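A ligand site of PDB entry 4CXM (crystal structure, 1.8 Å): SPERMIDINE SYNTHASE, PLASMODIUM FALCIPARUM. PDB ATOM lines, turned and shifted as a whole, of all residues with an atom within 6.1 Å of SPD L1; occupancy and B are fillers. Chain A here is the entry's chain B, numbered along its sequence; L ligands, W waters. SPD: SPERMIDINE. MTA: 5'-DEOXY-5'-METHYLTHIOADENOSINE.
The side-chain carboxylate (OD2) of Asp 161 lies within salt-bridge range of a nitrogen (N1) of SPD L1 (2.9 Å).
OD1 of Asp 89 lies within salt-bridge range of N10 of SPD L1 (2.6 Å).
The backbone NH (N) of Gly 87 sits close to a sulfur (S5') of MTA L2 (3.7 Å).
The backbone NH of Ser 160 sits close to an oxygen (O4') of MTA L2.
N6 of SPD L1 lies within hydrogen-bond range of O of Ser 159, 2.9 Å away.
The side-chain carboxylate (OD2) of Asp 158 is in salt-bridge range of a nitrogen (N10) of SPD L1 (2.6 Å).
A ring nitrogen (NE2) of His 65 is in hydrogen-bond range of a nitrogen (N10) of SPD L1 (2.8 Å).
A sulfur (S5') of MTA L2 lies close to a nitrogen (N10) of SPD L1, 3.5 Å away.
The side-chain hydroxyl (OH) of Tyr 226 sits at hydrogen-bond distance from the backbone carbonyl oxygen (O) of Gln 55.
OE2 of Glu 8 lies within hydrogen-bond range of N of Ile 54, 2.8 Å away.
The side-chain carboxylate (OD2) of Asp 89 lies within hydrogen-bond range of a ring nitrogen (NE2) of His 65 (3.3 Å).
OD2 of Asp 89 is in hydrogen-bond range of N of Gly 91 (2.9 Å).
The backbone carbonyl oxygen (O) of Asp 158 sits at hydrogen-bond distance from the backbone NH (N) of Gly 87 (3.0 Å).
O of Ser 159 is in hydrogen-bond range of NE2 of Gln 191, 3.0 Å away.
OE1 of Gln 55 sits close to O of Val 53 (3.1 Å).
The side-chain hydroxyl (OH) of Tyr 64 is in hydrogen-bond range of the side-chain carboxylate (OD1) of Asp 158, 2.6 Å away.
CG1 of Val 53 touches N1 of SPD L1, at 3.7 Å.
Ile 54 touches SPD L1 (O to C2, 3.5 Å).
Gln 55 touches SPD L1 (O to C8, 2.8 Å).
Tyr 64 touches SPD L1.
OH of Tyr 226 touches C5 of SPD L1, 3.3 Å away.
Hydrophobic or aromatic side chains that line SPD L1: Val 53, Tyr 64, His 65 and Tyr 226.
Along chain A the residues within 4 Å of SPD L1 span positions 53 to 226.
The nearest printed residue that does not touch SPD L1 is Ile 231 (4.02 Å).
Water W2 lies within hydrogen-bond range of the side-chain carboxylate (OE2) of Glu 8 (2.7 Å), the backbone carbonyl oxygen (O) of Ile 54 (2.8 Å) and a nitrogen (N1) of SPD L1 (2.9 Å).
Water W1 lies within hydrogen-bond range of OD2 of Asp 89 (2.7 Å), OD2 of Asp 158 (2.8 Å), N of Ile 92 (2.9 Å), N of Gly 91 (3.2 Å), N10 of SPD L1 (3.3 Å) and NE2 of His 65 (3.4 Å).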
ATOM      1  N   GLU A   8      -5.559   0.978   1.655  1.00  0.00           N
ATOM      2  CA  GLU A   8      -6.566   0.370   2.495  1.00  0.00           C
ATOM      3  C   GLU A   8      -5.803  -0.295   3.630  1.00  0.00           C
ATOM      4  O   GLU A   8      -5.086  -1.250   3.387  1.00  0.00           O
ATOM      5  CB  GLU A   8      -7.347  -0.716   1.729  1.00  0.00           C
ATOM      6  CG  GLU A   8      -8.412  -1.425   2.550  1.00  0.00           C
ATOM      7  CD  GLU A   8      -8.993  -2.637   1.863  1.00  0.00           C
ATOM      8  OE1 GLU A   8      -8.161  -3.541   1.612  1.00  0.00           O
ATOM      9  OE2 GLU A   8     -10.257  -2.722   1.661  1.00  0.00           O
ATOM     10  N   TRP A  13      -7.144  -6.286   9.640  1.00  0.00           N
ATOM     11  CA  TRP A  13      -6.050  -7.004   8.989  1.00  0.00           C
ATOM     12  C   TRP A  13      -4.683  -6.251   9.184  1.00  0.00           C
ATOM     13  O   TRP A  13      -4.084  -5.701   8.281  1.00  0.00           O
ATOM     14  CB  TRP A  13      -6.319  -7.286   7.522  1.00  0.00           C
ATOM     15  CG  TRP A  13      -6.883  -6.163   6.692  1.00  0.00           C
ATOM     16  CD1 TRP A  13      -6.202  -5.275   6.048  1.00  0.00           C
ATOM     17  CD2 TRP A  13      -8.272  -5.900   6.429  1.00  0.00           C
ATOM     18  NE1 TRP A  13      -7.013  -4.385   5.418  1.00  0.00           N
ATOM     19  CE2 TRP A  13      -8.314  -4.801   5.585  1.00  0.00           C
ATOM     20  CE3 TRP A  13      -9.442  -6.545   6.768  1.00  0.00           C
ATOM     21  CZ2 TRP A  13      -9.508  -4.259   5.099  1.00  0.00           C
ATOM     22  CZ3 TRP A  13     -10.686  -6.002   6.312  1.00  0.00           C
ATOM     23  CH2 TRP A  13     -10.672  -4.833   5.498  1.00  0.00           C
ATOM     24  N   VAL A  53     -12.654   1.022   3.505  1.00  0.00           N
ATOM     25  CA  VAL A  53     -12.517  -0.379   3.048  1.00  0.00           C
ATOM     26  C   VAL A  53     -13.086  -0.459   1.628  1.00  0.00           C
ATOM     27  O   VAL A  53     -14.228  -0.112   1.410  1.00  0.00           O
ATOM     28  CB  VAL A  53     -13.245  -1.339   3.995  1.00  0.00           C
ATOM     29  CG1 VAL A  53     -13.241  -2.815   3.506  1.00  0.00           C
ATOM     30  CG2 VAL A  53     -12.728  -1.267   5.410  1.00  0.00           C
ATOM     31  N   ILE A  54     -12.324  -1.024   0.709  1.00  0.00           N
ATOM     32  CA  ILE A  54     -12.832  -1.355  -0.640  1.00  0.00           C
ATOM     33  C   ILE A  54     -14.038  -2.260  -0.618  1.00  0.00           C
ATOM     34  O   ILE A  54     -14.021  -3.378  -0.088  1.00  0.00           O
ATOM     35  CB  ILE A  54     -11.708  -1.964  -1.535  1.00  0.00           C
ATOM     36  CG1 ILE A  54     -10.513  -0.971  -1.649  1.00  0.00           C
ATOM     37  CG2 ILE A  54     -12.196  -2.219  -2.960  1.00  0.00           C
ATOM     38  CD1 ILE A  54      -9.201  -1.534  -2.185  1.00  0.00           C
ATOM     39  N   GLN A  55     -15.092  -1.816  -1.232  1.00  0.00           N
ATOM     40  CA  GLN A  55     -16.250  -2.679  -1.352  1.00  0.00           C
ATOM     41  C   GLN A  55     -16.325  -3.308  -2.696  1.00  0.00           C
ATOM     42  O   GLN A  55     -16.798  -4.424  -2.818  1.00  0.00           O
ATOM     43  CB  GLN A  55     -17.497  -1.786  -1.226  1.00  0.00           C
ATOM     44  CG  GLN A  55     -17.625  -1.085   0.093  1.00  0.00           C
ATOM     45  CD  GLN A  55     -17.574  -2.015   1.251  1.00  0.00           C
ATOM     46  OE1 GLN A  55     -16.603  -2.009   2.069  1.00  0.00           O
ATOM     47  NE2 GLN A  55     -18.576  -2.840   1.344  1.00  0.00           N
ATOM     48  N   LEU A  56     -15.948  -2.570  -3.718  1.00  0.00           N
ATOM     49  CA  LEU A  56     -15.869  -3.071  -5.096  1.00  0.00           C
ATOM     50  C   LEU A  56     -15.008  -2.271  -6.008  1.00  0.00           C
ATOM     51  O   LEU A  56     -14.785  -1.134  -5.756  1.00  0.00           O
ATOM     52  CB  LEU A  56     -17.260  -3.324  -5.728  1.00  0.00           C
ATOM     53  CG  LEU A  56     -18.088  -2.063  -5.861  1.00  0.00           C
ATOM     54  CD1 LEU A  56     -17.688  -1.301  -7.106  1.00  0.00           C
ATOM     55  CD2 LEU A  56     -19.568  -2.527  -5.952  1.00  0.00           C
ATOM     56  N   TYR A  64     -17.120 -11.715  -7.273  1.00  0.00           N
ATOM     57  CA  TYR A  64     -17.857 -11.756  -6.056  1.00  0.00           C
ATOM     58  C   TYR A  64     -19.386 -11.875  -6.324  1.00  0.00           C
ATOM     59  O   TYR A  64     -20.105 -12.729  -5.773  1.00  0.00           O
ATOM     60  CB  TYR A  64     -17.490 -10.506  -5.226  1.00  0.00           C
ATOM     61  CG  TYR A  64     -18.313 -10.395  -3.968  1.00  0.00           C
ATOM     62  CD1 TYR A  64     -18.067 -11.260  -2.864  1.00  0.00           C
ATOM     63  CD2 TYR A  64     -19.284  -9.424  -3.850  1.00  0.00           C
ATOM     64  CE1 TYR A  64     -18.770 -11.084  -1.686  1.00  0.00           C
ATOM     65  CE2 TYR A  64     -20.011  -9.227  -2.690  1.00  0.00           C
ATOM     66  CZ  TYR A  64     -19.754 -10.070  -1.615  1.00  0.00           C
ATOM     67  OH  TYR A  64     -20.436  -9.945  -0.454  1.00  0.00           O
ATOM     68  N   HIS A  65     -19.867 -10.985  -7.154  1.00  0.00           N
ATOM     69  CA  HIS A  65     -21.330 -10.944  -7.390  1.00  0.00           C
ATOM     70  C   HIS A  65     -21.834 -12.214  -8.046  1.00  0.00           C
ATOM     71  O   HIS A  65     -22.896 -12.695  -7.701  1.00  0.00           O
ATOM     72  CB  HIS A  65     -21.761  -9.679  -8.114  1.00  0.00           C
ATOM     73  CG  HIS A  65     -21.499  -8.458  -7.304  1.00  0.00           C
ATOM     74  ND1 HIS A  65     -20.842  -7.381  -7.811  1.00  0.00           N
ATOM     75  CD2 HIS A  65     -21.867  -8.134  -6.058  1.00  0.00           C
ATOM     76  CE1 HIS A  65     -20.700  -6.455  -6.859  1.00  0.00           C
ATOM     77  NE2 HIS A  65     -21.316  -6.894  -5.785  1.00  0.00           N
ATOM     78  N   GLY A  87     -25.743  -4.913  -0.021  1.00  0.00           N
ATOM     79  CA  GLY A  87     -25.716  -4.930  -1.504  1.00  0.00           C
ATOM     80  C   GLY A  87     -26.271  -3.711  -2.215  1.00  0.00           C
ATOM     81  O   GLY A  87     -26.741  -3.798  -3.309  1.00  0.00           O
ATOM     82  N   GLY A  88     -26.180  -2.531  -1.574  1.00  0.00           N
ATOM     83  CA  GLY A  88     -26.683  -1.301  -2.176  1.00  0.00           C
ATOM     84  C   GLY A  88     -26.144  -0.979  -3.553  1.00  0.00           C
ATOM     85  O   GLY A  88     -26.797  -0.260  -4.329  1.00  0.00           O
ATOM     86  N   ASP A  89     -24.947  -1.479  -3.909  1.00  0.00           N
ATOM     87  CA  ASP A  89     -24.384  -1.202  -5.223  1.00  0.00           C
ATOM     88  C   ASP A  89     -25.257  -1.826  -6.317  1.00  0.00           C
ATOM     89  O   ASP A  89     -25.221  -1.414  -7.430  1.00  0.00           O
ATOM     90  CB  ASP A  89     -22.984  -1.791  -5.346  1.00  0.00           C
ATOM     91  CG  ASP A  89     -22.948  -3.226  -4.820  1.00  0.00           C
ATOM     92  OD1 ASP A  89     -22.811  -3.380  -3.603  1.00  0.00           O
ATOM     93  OD2 ASP A  89     -23.092  -4.159  -5.619  1.00  0.00           O
ATOM     94  N   GLY A  90     -25.945  -2.928  -5.934  1.00  0.00           N
ATOM     95  CA  GLY A  90     -26.884  -3.656  -6.843  1.00  0.00           C
ATOM     96  C   GLY A  90     -26.332  -4.830  -7.662  1.00  0.00           C
ATOM     97  O   GLY A  90     -27.030  -5.433  -8.473  1.00  0.00           O
ATOM     98  N   GLY A  91     -25.066  -5.142  -7.447  1.00  0.00           N
ATOM     99  CA  GLY A  91     -24.370  -6.225  -8.192  1.00  0.00           C
ATOM    100  C   GLY A  91     -25.064  -7.557  -7.989  1.00  0.00           C
ATOM    101  O   GLY A  91     -25.360  -8.192  -8.964  1.00  0.00           O
ATOM    102  N   ILE A  92     -25.461  -7.869  -6.767  1.00  0.00           N
ATOM    103  CA  ILE A  92     -26.256  -9.092  -6.539  1.00  0.00           C
ATOM    104  C   ILE A  92     -27.618  -9.040  -7.292  1.00  0.00           C
ATOM    105  O   ILE A  92     -28.044  -9.998  -7.981  1.00  0.00           O
ATOM    106  CB  ILE A  92     -26.495  -9.394  -5.071  1.00  0.00           C
ATOM    107  CG1 ILE A  92     -25.149  -9.512  -4.291  1.00  0.00           C
ATOM    108  CG2 ILE A  92     -27.323 -10.716  -4.891  1.00  0.00           C
ATOM    109  CD1 ILE A  92     -24.268 -10.629  -4.765  1.00  0.00           C
ATOM    110  N   ASP A 158     -24.917  -9.665   1.603  1.00  0.00           N
ATOM    111  CA  ASP A 158     -23.893  -8.936   0.950  1.00  0.00           C
ATOM    112  C   ASP A 158     -23.541  -7.690   1.825  1.00  0.00           C
ATOM    113  O   ASP A 158     -23.750  -6.549   1.425  1.00  0.00           O
ATOM    114  CB  ASP A 158     -24.246  -8.486  -0.451  1.00  0.00           C
ATOM    115  CG  ASP A 158     -23.071  -7.751  -1.113  1.00  0.00           C
ATOM    116  OD1 ASP A 158     -21.915  -7.786  -0.562  1.00  0.00           O
ATOM    117  OD2 ASP A 158     -23.267  -7.143  -2.198  1.00  0.00           O
ATOM    118  N   SER A 159     -23.003  -7.939   2.991  1.00  0.00           N
ATOM    119  CA  SER A 159     -22.742  -6.878   3.952  1.00  0.00           C
ATOM    120  C   SER A 159     -21.346  -6.255   3.744  1.00  0.00           C
ATOM    121  O   SER A 159     -20.429  -6.848   3.152  1.00  0.00           O
ATOM    122  CB  SER A 159     -22.734  -7.485   5.409  1.00  0.00           C
ATOM    123  OG  SER A 159     -21.803  -8.588   5.375  1.00  0.00           O
ATOM    124  N   SER A 160     -21.203  -5.062   4.320  1.00  0.00           N
ATOM    125  CA  SER A 160     -19.889  -4.543   4.587  1.00  0.00           C
ATOM    126  C   SER A 160     -19.357  -5.288   5.820  1.00  0.00           C
ATOM    127  O   SER A 160     -20.004  -6.213   6.346  1.00  0.00           O
ATOM    128  CB  SER A 160     -19.984  -3.020   4.783  1.00  0.00           C
ATOM    129  OG  SER A 160     -20.999  -2.738   5.737  1.00  0.00           O
ATOM    130  N   ASP A 161     -18.168  -4.893   6.246  1.00  0.00           N
ATOM    131  CA  ASP A 161     -17.414  -5.578   7.327  1.00  0.00           C
ATOM    132  C   ASP A 161     -17.923  -5.238   8.742  1.00  0.00           C
ATOM    133  O   ASP A 161     -18.667  -4.252   8.910  1.00  0.00           O
ATOM    134  CB  ASP A 161     -15.961  -5.251   7.189  1.00  0.00           C
ATOM    135  CG  ASP A 161     -15.357  -5.883   5.939  1.00  0.00           C
ATOM    136  OD1 ASP A 161     -15.630  -7.076   5.630  1.00  0.00           O
ATOM    137  OD2 ASP A 161     -14.710  -5.148   5.221  1.00  0.00           O
ATOM    138  N   GLN A 191     -21.234 -13.268   3.035  1.00  0.00           N
ATOM    139  CA  GLN A 191     -19.839 -12.899   2.889  1.00  0.00           C
ATOM    140  C   GLN A 191     -19.208 -13.207   4.216  1.00  0.00           C
ATOM    141  O   GLN A 191     -19.818 -12.912   5.278  1.00  0.00           O
ATOM    142  CB  GLN A 191     -19.867 -11.410   2.549  1.00  0.00           C
ATOM    143  CG  GLN A 191     -18.727 -10.520   2.508  1.00  0.00           C
ATOM    144  CD  GLN A 191     -18.232 -10.075   3.862  1.00  0.00           C
ATOM    145  OE1 GLN A 191     -17.333 -10.707   4.320  1.00  0.00           O
ATOM    146  NE2 GLN A 191     -18.723  -8.917   4.432  1.00  0.00           N
ATOM    147  N   TYR A 226      -9.978  -7.434  -2.451  1.00  0.00           N
ATOM    148  CA  TYR A 226     -10.276  -7.661  -1.048  1.00  0.00           C
ATOM    149  C   TYR A 226      -9.002  -8.134  -0.346  1.00  0.00           C
ATOM    150  O   TYR A 226      -8.100  -8.701  -1.010  1.00  0.00           O
ATOM    151  CB  TYR A 226     -11.374  -8.679  -0.866  1.00  0.00           C
ATOM    152  CG  TYR A 226     -12.803  -8.202  -1.297  1.00  0.00           C
ATOM    153  CD1 TYR A 226     -13.152  -6.868  -1.338  1.00  0.00           C
ATOM    154  CD2 TYR A 226     -13.768  -9.113  -1.644  1.00  0.00           C
ATOM    155  CE1 TYR A 226     -14.453  -6.457  -1.653  1.00  0.00           C
ATOM    156  CE2 TYR A 226     -15.056  -8.711  -2.014  1.00  0.00           C
ATOM    157  CZ  TYR A 226     -15.387  -7.384  -2.043  1.00  0.00           C
ATOM    158  OH  TYR A 226     -16.680  -7.013  -2.449  1.00  0.00           O
ATOM    159  N   PRO A 227      -8.861  -7.835   0.952  1.00  0.00           N
ATOM    160  CA  PRO A 227      -7.618  -8.188   1.600  1.00  0.00           C
ATOM    161  C   PRO A 227      -7.245  -9.657   1.487  1.00  0.00           C
ATOM    162  O   PRO A 227      -8.143 -10.485   1.657  1.00  0.00           O
ATOM    163  CB  PRO A 227      -7.914  -7.868   3.084  1.00  0.00           C
ATOM    164  CG  PRO A 227      -9.229  -7.291   3.201  1.00  0.00           C
ATOM    165  CD  PRO A 227      -9.860  -7.254   1.875  1.00  0.00           C
ATOM    166  N   ILE A 231     -12.240 -13.939  -0.615  1.00  0.00           N
ATOM    167  CA  ILE A 231     -13.233 -13.751   0.389  1.00  0.00           C
ATOM    168  C   ILE A 231     -14.002 -15.087   0.462  1.00  0.00           C
ATOM    169  O   ILE A 231     -14.088 -15.745  -0.466  1.00  0.00           O
ATOM    170  CB  ILE A 231     -14.114 -12.580   0.106  1.00  0.00           C
ATOM    171  CG1 ILE A 231     -14.998 -12.237   1.314  1.00  0.00           C
ATOM    172  CG2 ILE A 231     -14.995 -12.855  -1.106  1.00  0.00           C
ATOM    173  CD1 ILE A 231     -15.657 -10.882   1.228  1.00  0.00           C
HETATM  174  N1  SPD L   1     -13.748  -6.414   2.776  1.00  0.00           N
HETATM  175  C2  SPD L   1     -14.959  -5.929   2.073  1.00  0.00           C
HETATM  176  C3  SPD L   1     -16.058  -6.911   1.707  1.00  0.00           C
HETATM  177  C4  SPD L   1     -17.310  -6.098   1.279  1.00  0.00           C
HETATM  178  C5  SPD L   1     -18.243  -6.977   0.481  1.00  0.00           C
HETATM  179  N6  SPD L   1     -19.574  -6.405   0.409  1.00  0.00           N
HETATM  180  C7  SPD L   1     -20.015  -5.374  -0.516  1.00  0.00           C
HETATM  181  C8  SPD L   1     -19.378  -5.090  -1.874  1.00  0.00           C
HETATM  182  C9  SPD L   1     -20.007  -5.692  -3.172  1.00  0.00           C
HETATM  183  N10 SPD L   1     -21.455  -5.628  -3.286  1.00  0.00           N
HETATM  184  CS  MTA L   2     -21.822  -2.106  -0.767  1.00  0.00           C
HETATM  185  S5' MTA L   2     -22.264  -3.761  -0.403  1.00  0.00           S
HETATM  186  C5' MTA L   2     -22.343  -3.699   1.373  1.00  0.00           C
HETATM  187  C4' MTA L   2     -23.478  -2.900   2.021  1.00  0.00           C
HETATM  188  O4' MTA L   2     -24.002  -3.311   3.265  1.00  0.00           O
HETATM  189  C2' MTA L   2     -23.804  -1.087   3.495  1.00  0.00           C
HETATM  190  O2' MTA L   2     -24.429   0.197   3.663  1.00  0.00           O
HETATM  191  C3' MTA L   2     -23.311  -1.403   2.091  1.00  0.00           C
HETATM  192  O3' MTA L   2     -23.971  -0.657   1.088  1.00  0.00           O
HETATM  193  C1' MTA L   2     -24.780  -2.233   3.767  1.00  0.00           C
HETATM  194  N9  MTA L   2     -25.086  -2.436   5.154  1.00  0.00           N
HETATM  195  C8  MTA L   2     -24.210  -2.364   6.201  1.00  0.00           C
HETATM  196  N7  MTA L   2     -24.830  -2.628   7.351  1.00  0.00           N
HETATM  197  C5  MTA L   2     -26.086  -2.933   7.043  1.00  0.00           C
HETATM  198  C6  MTA L   2     -27.237  -3.326   7.813  1.00  0.00           C
HETATM  199  N6  MTA L   2     -27.162  -3.453   9.139  1.00  0.00           N
HETATM  200  N1  MTA L   2     -28.400  -3.544   7.127  1.00  0.00           N
HETATM  201  C2  MTA L   2     -28.468  -3.387   5.799  1.00  0.00           C
HETATM  202  N3  MTA L   2     -27.455  -3.065   5.048  1.00  0.00           N
HETATM  203  C4  MTA L   2     -26.243  -2.787   5.615  1.00  0.00           C
HETATM  204  O   HOH W   1     -24.458  -6.240  -4.531  1.00  0.00           O
HETATM  205  O   HOH W   2     -11.933  -4.772   1.133  1.00  0.00           O
